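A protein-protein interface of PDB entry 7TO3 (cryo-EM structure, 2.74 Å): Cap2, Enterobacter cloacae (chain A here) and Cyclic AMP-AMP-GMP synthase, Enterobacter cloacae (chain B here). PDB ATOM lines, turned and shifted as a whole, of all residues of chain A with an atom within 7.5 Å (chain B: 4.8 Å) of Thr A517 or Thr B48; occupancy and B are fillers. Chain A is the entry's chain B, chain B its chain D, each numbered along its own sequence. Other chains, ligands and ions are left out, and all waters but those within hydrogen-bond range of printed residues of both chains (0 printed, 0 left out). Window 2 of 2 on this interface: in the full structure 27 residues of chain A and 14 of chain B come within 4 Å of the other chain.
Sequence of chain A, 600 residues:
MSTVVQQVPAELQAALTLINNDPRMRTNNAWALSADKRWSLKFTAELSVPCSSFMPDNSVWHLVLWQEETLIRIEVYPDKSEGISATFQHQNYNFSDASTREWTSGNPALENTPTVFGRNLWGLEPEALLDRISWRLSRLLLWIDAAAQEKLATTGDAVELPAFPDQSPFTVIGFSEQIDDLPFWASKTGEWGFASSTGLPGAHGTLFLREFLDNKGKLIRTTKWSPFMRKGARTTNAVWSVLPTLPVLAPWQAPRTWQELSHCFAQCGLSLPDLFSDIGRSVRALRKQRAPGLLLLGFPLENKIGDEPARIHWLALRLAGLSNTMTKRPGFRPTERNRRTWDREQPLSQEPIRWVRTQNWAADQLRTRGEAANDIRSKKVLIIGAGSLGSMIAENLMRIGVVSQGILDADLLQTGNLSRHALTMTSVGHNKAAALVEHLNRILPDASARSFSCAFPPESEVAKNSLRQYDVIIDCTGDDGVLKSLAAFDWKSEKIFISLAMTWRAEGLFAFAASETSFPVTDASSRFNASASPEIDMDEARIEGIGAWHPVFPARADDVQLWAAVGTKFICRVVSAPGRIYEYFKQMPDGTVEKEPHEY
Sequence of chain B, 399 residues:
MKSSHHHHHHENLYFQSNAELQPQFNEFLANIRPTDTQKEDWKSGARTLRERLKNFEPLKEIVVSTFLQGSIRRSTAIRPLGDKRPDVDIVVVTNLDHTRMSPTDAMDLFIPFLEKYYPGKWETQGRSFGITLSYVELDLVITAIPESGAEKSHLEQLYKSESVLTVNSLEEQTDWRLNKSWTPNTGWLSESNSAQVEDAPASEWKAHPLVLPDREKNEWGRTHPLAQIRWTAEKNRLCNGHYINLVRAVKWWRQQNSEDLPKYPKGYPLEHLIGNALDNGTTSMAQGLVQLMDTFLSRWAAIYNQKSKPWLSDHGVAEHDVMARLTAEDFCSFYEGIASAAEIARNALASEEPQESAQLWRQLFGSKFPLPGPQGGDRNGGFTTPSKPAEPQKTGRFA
The guanidinium group of Arg B52 lies within salt-bridge range of the side-chain carboxylate of Glu A494 (3.0 Å).
The side-chain hydroxyl (OG1) of Thr B48 lies within hydrogen-bond range of the side-chain carboxylate (OE1) of Glu A516.
The side-chain carboxylate (OE1) of Glu A516 sits close to the backbone carbonyl oxygen (O) of Ser B44 (3.2 Å).
OD1 of Asp A490 lies within hydrogen-bond range of N of Lys A492, at 3.5 Å.
The side-chain hydroxyl (OG) of Ser A515 is in hydrogen-bond range of the side-chain carboxylate (OE2) of Glu A494 (3.2 Å).
The backbone NH (N) of Lys A495 sits at hydrogen-bond distance from the backbone carbonyl oxygen (O) of Glu A516, 2.9 Å away.
O of Ser B44 lies within hydrogen-bond range of OG1 of Thr B48, 2.7 Å away.
Lys A492 touches Glu B51 (O to OE1, 3.8 Å).
Gly B45 touches Glu A516.
Thr B48 touches Thr A517.
Printed residues of chain B within 4 Å of Glu A494: Arg B52.
Thr A517 touches one residue of chain B.
Of the printed residues of chain A, Ser B44 touches Glu A516 (3.2 Å).
Of the printed residues of chain A, Gly B45 touches Glu A516.
Printed residues of chain A that touch a printed residue of chain B: Lys A492, Glu A494, Glu A516 and Thr A517.
Of the 9 printed residues of chain B, 5 touch a printed residue of chain A.
Along chain B the printed residues that touch a printed residue of chain A span positions 44 to 52.
Among the printed residues, Asp or Glu carboxylates within 4 Å of a Lys or Arg side-chain nitrogen of the other chain: Glu A494 with Arg B52 (3.0 Å).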
ATOM      1  N   LEU A 486       7.959  23.397  -4.163  1.00  0.00           N
ATOM      2  CA  LEU A 486       9.043  24.304  -3.802  1.00  0.00           C
ATOM      3  C   LEU A 486       9.848  23.755  -2.631  1.00  0.00           C
ATOM      4  O   LEU A 486      11.082  23.834  -2.623  1.00  0.00           O
ATOM      5  CB  LEU A 486       8.481  25.685  -3.467  1.00  0.00           C
ATOM      6  CG  LEU A 486       8.204  26.622  -4.644  1.00  0.00           C
ATOM      7  CD1 LEU A 486       7.376  27.816  -4.195  1.00  0.00           C
ATOM      8  CD2 LEU A 486       9.501  27.079  -5.287  1.00  0.00           C
ATOM      9  N   ALA A 487       9.165  23.195  -1.631  1.00  0.00           N
ATOM     10  CA  ALA A 487       9.858  22.582  -0.506  1.00  0.00           C
ATOM     11  C   ALA A 487      10.557  21.288  -0.897  1.00  0.00           C
ATOM     12  O   ALA A 487      11.537  20.907  -0.247  1.00  0.00           O
ATOM     13  CB  ALA A 487       8.879  22.319   0.639  1.00  0.00           C
ATOM     14  N   PHE A 489      12.144  20.813  -3.733  1.00  0.00           N
ATOM     15  CA  PHE A 489      13.168  21.099  -4.731  1.00  0.00           C
ATOM     16  C   PHE A 489      14.495  21.436  -4.062  1.00  0.00           C
ATOM     17  O   PHE A 489      14.535  22.138  -3.049  1.00  0.00           O
ATOM     18  CB  PHE A 489      12.728  22.254  -5.633  1.00  0.00           C
ATOM     19  CG  PHE A 489      13.564  22.411  -6.872  1.00  0.00           C
ATOM     20  CD1 PHE A 489      13.305  21.648  -7.999  1.00  0.00           C
ATOM     21  CD2 PHE A 489      14.603  23.326  -6.914  1.00  0.00           C
ATOM     22  CE1 PHE A 489      14.069  21.792  -9.143  1.00  0.00           C
ATOM     23  CE2 PHE A 489      15.371  23.475  -8.054  1.00  0.00           C
ATOM     24  CZ  PHE A 489      15.104  22.706  -9.170  1.00  0.00           C
ATOM     25  N   ASP A 490      15.583  20.928  -4.641  1.00  0.00           N
ATOM     26  CA  ASP A 490      16.930  21.179  -4.138  1.00  0.00           C
ATOM     27  C   ASP A 490      17.499  22.405  -4.844  1.00  0.00           C
ATOM     28  O   ASP A 490      17.828  22.349  -6.033  1.00  0.00           O
ATOM     29  CB  ASP A 490      17.821  19.957  -4.353  1.00  0.00           C
ATOM     30  CG  ASP A 490      19.156  20.075  -3.643  1.00  0.00           C
ATOM     31  OD1 ASP A 490      19.280  20.931  -2.742  1.00  0.00           O
ATOM     32  OD2 ASP A 490      20.083  19.311  -3.985  1.00  0.00           O
ATOM     33  N   TRP A 491      17.618  23.512  -4.111  1.00  0.00           N
ATOM     34  CA  TRP A 491      18.132  24.753  -4.676  1.00  0.00           C
ATOM     35  C   TRP A 491      19.644  24.882  -4.561  1.00  0.00           C
ATOM     36  O   TRP A 491      20.236  25.700  -5.274  1.00  0.00           O
ATOM     37  CB  TRP A 491      17.463  25.954  -4.002  1.00  0.00           C
ATOM     38  CG  TRP A 491      15.981  25.997  -4.214  1.00  0.00           C
ATOM     39  CD1 TRP A 491      15.016  25.562  -3.352  1.00  0.00           C
ATOM     40  CD2 TRP A 491      15.292  26.494  -5.367  1.00  0.00           C
ATOM     41  NE1 TRP A 491      13.770  25.762  -3.895  1.00  0.00           N
ATOM     42  CE2 TRP A 491      13.912  26.334  -5.133  1.00  0.00           C
ATOM     43  CE3 TRP A 491      15.709  27.062  -6.575  1.00  0.00           C
ATOM     44  CZ2 TRP A 491      12.948  26.719  -6.060  1.00  0.00           C
ATOM     45  CZ3 TRP A 491      14.749  27.445  -7.495  1.00  0.00           C
ATOM     46  CH2 TRP A 491      13.384  27.272  -7.233  1.00  0.00           C
ATOM     47  N   LYS A 492      20.275  24.109  -3.676  1.00  0.00           N
ATOM     48  CA  LYS A 492      21.721  24.005  -3.499  1.00  0.00           C
ATOM     49  C   LYS A 492      22.367  25.288  -2.987  1.00  0.00           C
ATOM     50  O   LYS A 492      23.601  25.350  -2.912  1.00  0.00           O
ATOM     51  CB  LYS A 492      22.434  23.573  -4.790  1.00  0.00           C
ATOM     52  CG  LYS A 492      22.005  22.206  -5.299  1.00  0.00           C
ATOM     53  CD  LYS A 492      22.753  21.821  -6.564  1.00  0.00           C
ATOM     54  CE  LYS A 492      22.405  20.406  -6.997  1.00  0.00           C
ATOM     55  NZ  LYS A 492      23.108  20.017  -8.251  1.00  0.00           N
ATOM     56  N   SER A 493      21.588  26.307  -2.631  1.00  0.00           N
ATOM     57  CA  SER A 493      22.133  27.536  -2.071  1.00  0.00           C
ATOM     58  C   SER A 493      21.004  28.299  -1.392  1.00  0.00           C
ATOM     59  O   SER A 493      19.827  27.959  -1.529  1.00  0.00           O
ATOM     60  CB  SER A 493      22.813  28.394  -3.144  1.00  0.00           C
ATOM     61  OG  SER A 493      21.886  28.821  -4.124  1.00  0.00           O
ATOM     62  N   GLU A 494      21.381  29.339  -0.651  1.00  0.00           N
ATOM     63  CA  GLU A 494      20.408  30.144   0.076  1.00  0.00           C
ATOM     64  C   GLU A 494      19.668  31.068  -0.883  1.00  0.00           C
ATOM     65  O   GLU A 494      20.286  31.738  -1.716  1.00  0.00           O
ATOM     66  CB  GLU A 494      21.100  30.956   1.171  1.00  0.00           C
ATOM     67  CG  GLU A 494      20.141  31.656   2.119  1.00  0.00           C
ATOM     68  CD  GLU A 494      20.856  32.415   3.218  1.00  0.00           C
ATOM     69  OE1 GLU A 494      22.081  32.224   3.375  1.00  0.00           O
ATOM     70  OE2 GLU A 494      20.194  33.203   3.927  1.00  0.00           O
ATOM     71  N   LYS A 495      18.343  31.102  -0.760  1.00  0.00           N
ATOM     72  CA  LYS A 495      17.486  31.892  -1.632  1.00  0.00           C
ATOM     73  C   LYS A 495      16.479  32.677  -0.802  1.00  0.00           C
ATOM     74  O   LYS A 495      16.224  32.379   0.370  1.00  0.00           O
ATOM     75  CB  LYS A 495      16.745  31.012  -2.649  1.00  0.00           C
ATOM     76  CG  LYS A 495      17.621  30.034  -3.412  1.00  0.00           C
ATOM     77  CD  LYS A 495      18.455  30.748  -4.463  1.00  0.00           C
ATOM     78  CE  LYS A 495      19.131  29.754  -5.392  1.00  0.00           C
ATOM     79  NZ  LYS A 495      20.095  30.416  -6.314  1.00  0.00           N
ATOM     80  N   ILE A 496      15.898  33.690  -1.444  1.00  0.00           N
ATOM     81  CA  ILE A 496      14.847  34.517  -0.862  1.00  0.00           C
ATOM     82  C   ILE A 496      13.528  34.118  -1.510  1.00  0.00           C
ATOM     83  O   ILE A 496      13.324  34.337  -2.712  1.00  0.00           O
ATOM     84  CB  ILE A 496      15.124  36.014  -1.060  1.00  0.00           C
ATOM     85  CG1 ILE A 496      16.571  36.349  -0.691  1.00  0.00           C
ATOM     86  CG2 ILE A 496      14.152  36.850  -0.238  1.00  0.00           C
ATOM     87  CD1 ILE A 496      16.967  37.773  -1.016  1.00  0.00           C
ATOM     88  N   PHE A 497      12.628  33.560  -0.706  1.00  0.00           N
ATOM     89  CA  PHE A 497      11.334  33.075  -1.164  1.00  0.00           C
ATOM     90  C   PHE A 497      10.253  34.061  -0.747  1.00  0.00           C
ATOM     91  O   PHE A 497      10.174  34.442   0.427  1.00  0.00           O
ATOM     92  CB  PHE A 497      11.030  31.694  -0.580  1.00  0.00           C
ATOM     93  CG  PHE A 497      12.019  30.636  -0.974  1.00  0.00           C
ATOM     94  CD1 PHE A 497      11.935  30.013  -2.207  1.00  0.00           C
ATOM     95  CD2 PHE A 497      13.032  30.264  -0.106  1.00  0.00           C
ATOM     96  CE1 PHE A 497      12.846  29.038  -2.569  1.00  0.00           C
ATOM     97  CE2 PHE A 497      13.945  29.290  -0.460  1.00  0.00           C
ATOM     98  CZ  PHE A 497      13.852  28.676  -1.694  1.00  0.00           C
ATOM     99  N   SER A 515      14.129  33.591   3.952  1.00  0.00           N
ATOM    100  CA  SER A 515      15.462  33.546   3.346  1.00  0.00           C
ATOM    101  C   SER A 515      16.172  32.293   3.851  1.00  0.00           C
ATOM    102  O   SER A 515      16.794  32.312   4.917  1.00  0.00           O
ATOM    103  CB  SER A 515      16.253  34.811   3.668  1.00  0.00           C
ATOM    104  OG  SER A 515      17.515  34.801   3.024  1.00  0.00           O
ATOM    105  N   GLU A 516      16.097  31.214   3.076  1.00  0.00           N
ATOM    106  CA  GLU A 516      16.626  29.920   3.504  1.00  0.00           C
ATOM    107  C   GLU A 516      17.036  29.119   2.273  1.00  0.00           C
ATOM    108  O   GLU A 516      16.813  29.537   1.133  1.00  0.00           O
ATOM    109  CB  GLU A 516      15.599  29.141   4.343  1.00  0.00           C
ATOM    110  CG  GLU A 516      15.278  29.724   5.713  1.00  0.00           C
ATOM    111  CD  GLU A 516      16.248  29.267   6.786  1.00  0.00           C
ATOM    112  OE1 GLU A 516      16.389  28.041   6.978  1.00  0.00           O
ATOM    113  OE2 GLU A 516      16.869  30.133   7.436  1.00  0.00           O
ATOM    114  N   THR A 517      17.643  27.956   2.514  1.00  0.00           N
ATOM    115  CA  THR A 517      17.949  27.005   1.453  1.00  0.00           C
ATOM    116  C   THR A 517      16.714  26.245   0.985  1.00  0.00           C
ATOM    117  O   THR A 517      16.628  25.880  -0.193  1.00  0.00           O
ATOM    118  CB  THR A 517      19.015  26.011   1.926  1.00  0.00           C
ATOM    119  OG1 THR A 517      20.098  26.724   2.537  1.00  0.00           O
ATOM    120  CG2 THR A 517      19.556  25.199   0.756  1.00  0.00           C
ATOM    121  N   SER A 518      15.755  26.009   1.879  1.00  0.00           N
ATOM    122  CA  SER A 518      14.520  25.316   1.550  1.00  0.00           C
ATOM    123  C   SER A 518      13.330  26.160   1.981  1.00  0.00           C
ATOM    124  O   SER A 518      13.405  26.918   2.952  1.00  0.00           O
ATOM    125  CB  SER A 518      14.453  23.935   2.218  1.00  0.00           C
ATOM    126  OG  SER A 518      13.294  23.228   1.812  1.00  0.00           O
ATOM    127  N   PHE A 519      12.230  26.022   1.248  1.00  0.00           N
ATOM    128  CA  PHE A 519      11.045  26.835   1.501  1.00  0.00           C
ATOM    129  C   PHE A 519      10.231  26.244   2.646  1.00  0.00           C
ATOM    130  O   PHE A 519       9.859  25.068   2.591  1.00  0.00           O
ATOM    131  CB  PHE A 519      10.185  26.932   0.244  1.00  0.00           C
ATOM    132  CG  PHE A 519       8.845  27.571   0.474  1.00  0.00           C
ATOM    133  CD1 PHE A 519       8.740  28.939   0.669  1.00  0.00           C
ATOM    134  CD2 PHE A 519       7.690  26.807   0.494  1.00  0.00           C
ATOM    135  CE1 PHE A 519       7.510  29.532   0.881  1.00  0.00           C
ATOM    136  CE2 PHE A 519       6.457  27.393   0.707  1.00  0.00           C
ATOM    137  CZ  PHE A 519       6.366  28.757   0.900  1.00  0.00           C
ATOM    138  N   PRO A 520       9.936  27.020   3.694  1.00  0.00           N
ATOM    139  CA  PRO A 520       9.072  26.531   4.778  1.00  0.00           C
ATOM    140  C   PRO A 520       7.605  26.606   4.378  1.00  0.00           C
ATOM    141  O   PRO A 520       7.051  27.691   4.179  1.00  0.00           O
ATOM    142  CB  PRO A 520       9.402  27.483   5.936  1.00  0.00           C
ATOM    143  CG  PRO A 520       9.819  28.752   5.271  1.00  0.00           C
ATOM    144  CD  PRO A 520      10.431  28.386   3.942  1.00  0.00           C
ATOM    145  N   SER B  44      15.589  22.909   8.355  1.00  0.00           N
ATOM    146  CA  SER B  44      15.997  24.010   7.491  1.00  0.00           C
ATOM    147  C   SER B  44      17.104  24.836   8.130  1.00  0.00           C
ATOM    148  O   SER B  44      18.031  25.281   7.441  1.00  0.00           O
ATOM    149  CB  SER B  44      14.790  24.888   7.160  1.00  0.00           C
ATOM    150  OG  SER B  44      14.234  25.449   8.336  1.00  0.00           O
ATOM    151  N   GLY B  45      17.025  25.060   9.446  1.00  0.00           N
ATOM    152  CA  GLY B  45      18.072  25.808  10.118  1.00  0.00           C
ATOM    153  C   GLY B  45      19.418  25.118  10.048  1.00  0.00           C
ATOM    154  O   GLY B  45      20.442  25.761   9.802  1.00  0.00           O
ATOM    155  N   ALA B  46      19.438  23.798  10.256  1.00  0.00           N
ATOM    156  CA  ALA B  46      20.693  23.061  10.158  1.00  0.00           C
ATOM    157  C   ALA B  46      21.284  23.168   8.757  1.00  0.00           C
ATOM    158  O   ALA B  46      22.485  23.428   8.593  1.00  0.00           O
ATOM    159  CB  ALA B  46      20.477  21.598  10.545  1.00  0.00           C
ATOM    160  N   ARG B  47      20.448  22.986   7.727  1.00  0.00           N
ATOM    161  CA  ARG B  47      20.966  23.064   6.361  1.00  0.00           C
ATOM    162  C   ARG B  47      21.500  24.459   6.039  1.00  0.00           C
ATOM    163  O   ARG B  47      22.581  24.602   5.445  1.00  0.00           O
ATOM    164  CB  ARG B  47      19.885  22.656   5.359  1.00  0.00           C
ATOM    165  CG  ARG B  47      19.412  21.221   5.512  1.00  0.00           C
ATOM    166  CD  ARG B  47      18.232  20.931   4.600  1.00  0.00           C
ATOM    167  NE  ARG B  47      17.328  19.940   5.170  1.00  0.00           N
ATOM    168  CZ  ARG B  47      16.131  19.649   4.680  1.00  0.00           C
ATOM    169  NH1 ARG B  47      15.659  20.259   3.605  1.00  0.00           N
ATOM    170  NH2 ARG B  47      15.390  18.724   5.282  1.00  0.00           N
ATOM    171  N   THR B  48      20.760  25.500   6.431  1.00  0.00           N
ATOM    172  CA  THR B  48      21.190  26.866   6.150  1.00  0.00           C
ATOM    173  C   THR B  48      22.488  27.192   6.878  1.00  0.00           C
ATOM    174  O   THR B  48      23.382  27.837   6.315  1.00  0.00           O
ATOM    175  CB  THR B  48      20.089  27.854   6.539  1.00  0.00           C
ATOM    176  OG1 THR B  48      18.845  27.437   5.962  1.00  0.00           O
ATOM    177  CG2 THR B  48      20.428  29.251   6.043  1.00  0.00           C
ATOM    178  N   LEU B  49      22.608  26.756   8.136  1.00  0.00           N
ATOM    179  CA  LEU B  49      23.839  26.988   8.881  1.00  0.00           C
ATOM    180  C   LEU B  49      25.018  26.288   8.222  1.00  0.00           C
ATOM    181  O   LEU B  49      26.115  26.851   8.142  1.00  0.00           O
ATOM    182  CB  LEU B  49      23.678  26.522  10.328  1.00  0.00           C
ATOM    183  CG  LEU B  49      24.934  26.628  11.196  1.00  0.00           C
ATOM    184  CD1 LEU B  49      25.287  28.085  11.454  1.00  0.00           C
ATOM    185  CD2 LEU B  49      24.756  25.874  12.504  1.00  0.00           C
ATOM    186  N   ARG B  50      24.811  25.058   7.743  1.00  0.00           N
ATOM    187  CA  ARG B  50      25.888  24.350   7.057  1.00  0.00           C
ATOM    188  C   ARG B  50      26.343  25.112   5.817  1.00  0.00           C
ATOM    189  O   ARG B  50      27.547  25.289   5.588  1.00  0.00           O
ATOM    190  CB  ARG B  50      25.436  22.939   6.682  1.00  0.00           C
ATOM    191  CG  ARG B  50      26.532  22.082   6.073  1.00  0.00           C
ATOM    192  CD  ARG B  50      25.967  20.781   5.535  1.00  0.00           C
ATOM    193  NE  ARG B  50      25.263  20.034   6.569  1.00  0.00           N
ATOM    194  CZ  ARG B  50      24.551  18.937   6.348  1.00  0.00           C
ATOM    195  NH1 ARG B  50      24.422  18.430   5.133  1.00  0.00           N
ATOM    196  NH2 ARG B  50      23.952  18.335   7.371  1.00  0.00           N
ATOM    197  N   GLU B  51      25.390  25.581   5.007  1.00  0.00           N
ATOM    198  CA  GLU B  51      25.758  26.310   3.794  1.00  0.00           C
ATOM    199  C   GLU B  51      26.508  27.598   4.127  1.00  0.00           C
ATOM    200  O   GLU B  51      27.541  27.909   3.516  1.00  0.00           O
ATOM    201  CB  GLU B  51      24.513  26.609   2.959  1.00  0.00           C
ATOM    202  CG  GLU B  51      24.799  27.409   1.695  1.00  0.00           C
ATOM    203  CD  GLU B  51      25.389  26.559   0.585  1.00  0.00           C
ATOM    204  OE1 GLU B  51      25.130  25.337   0.567  1.00  0.00           O
ATOM    205  OE2 GLU B  51      26.114  27.113  -0.268  1.00  0.00           O
ATOM    206  N   ARG B  52      26.007  28.353   5.109  1.00  0.00           N
ATOM    207  CA  ARG B  52      26.648  29.613   5.476  1.00  0.00           C
ATOM    208  C   ARG B  52      28.054  29.379   6.013  1.00  0.00           C
ATOM    209  O   ARG B  52      28.981  30.137   5.706  1.00  0.00           O
ATOM    210  CB  ARG B  52      25.795  30.360   6.502  1.00  0.00           C
ATOM    211  CG  ARG B  52      24.445  30.811   5.975  1.00  0.00           C
ATOM    212  CD  ARG B  52      23.545  31.272   7.106  1.00  0.00           C
ATOM    213  NE  ARG B  52      22.480  32.148   6.633  1.00  0.00           N
ATOM    214  CZ  ARG B  52      21.549  32.680   7.413  1.00  0.00           C
ATOM    215  NH1 ARG B  52      21.521  32.446   8.714  1.00  0.00           N
ATOM    216  NH2 ARG B  52      20.622  33.466   6.873  1.00  0.00           N
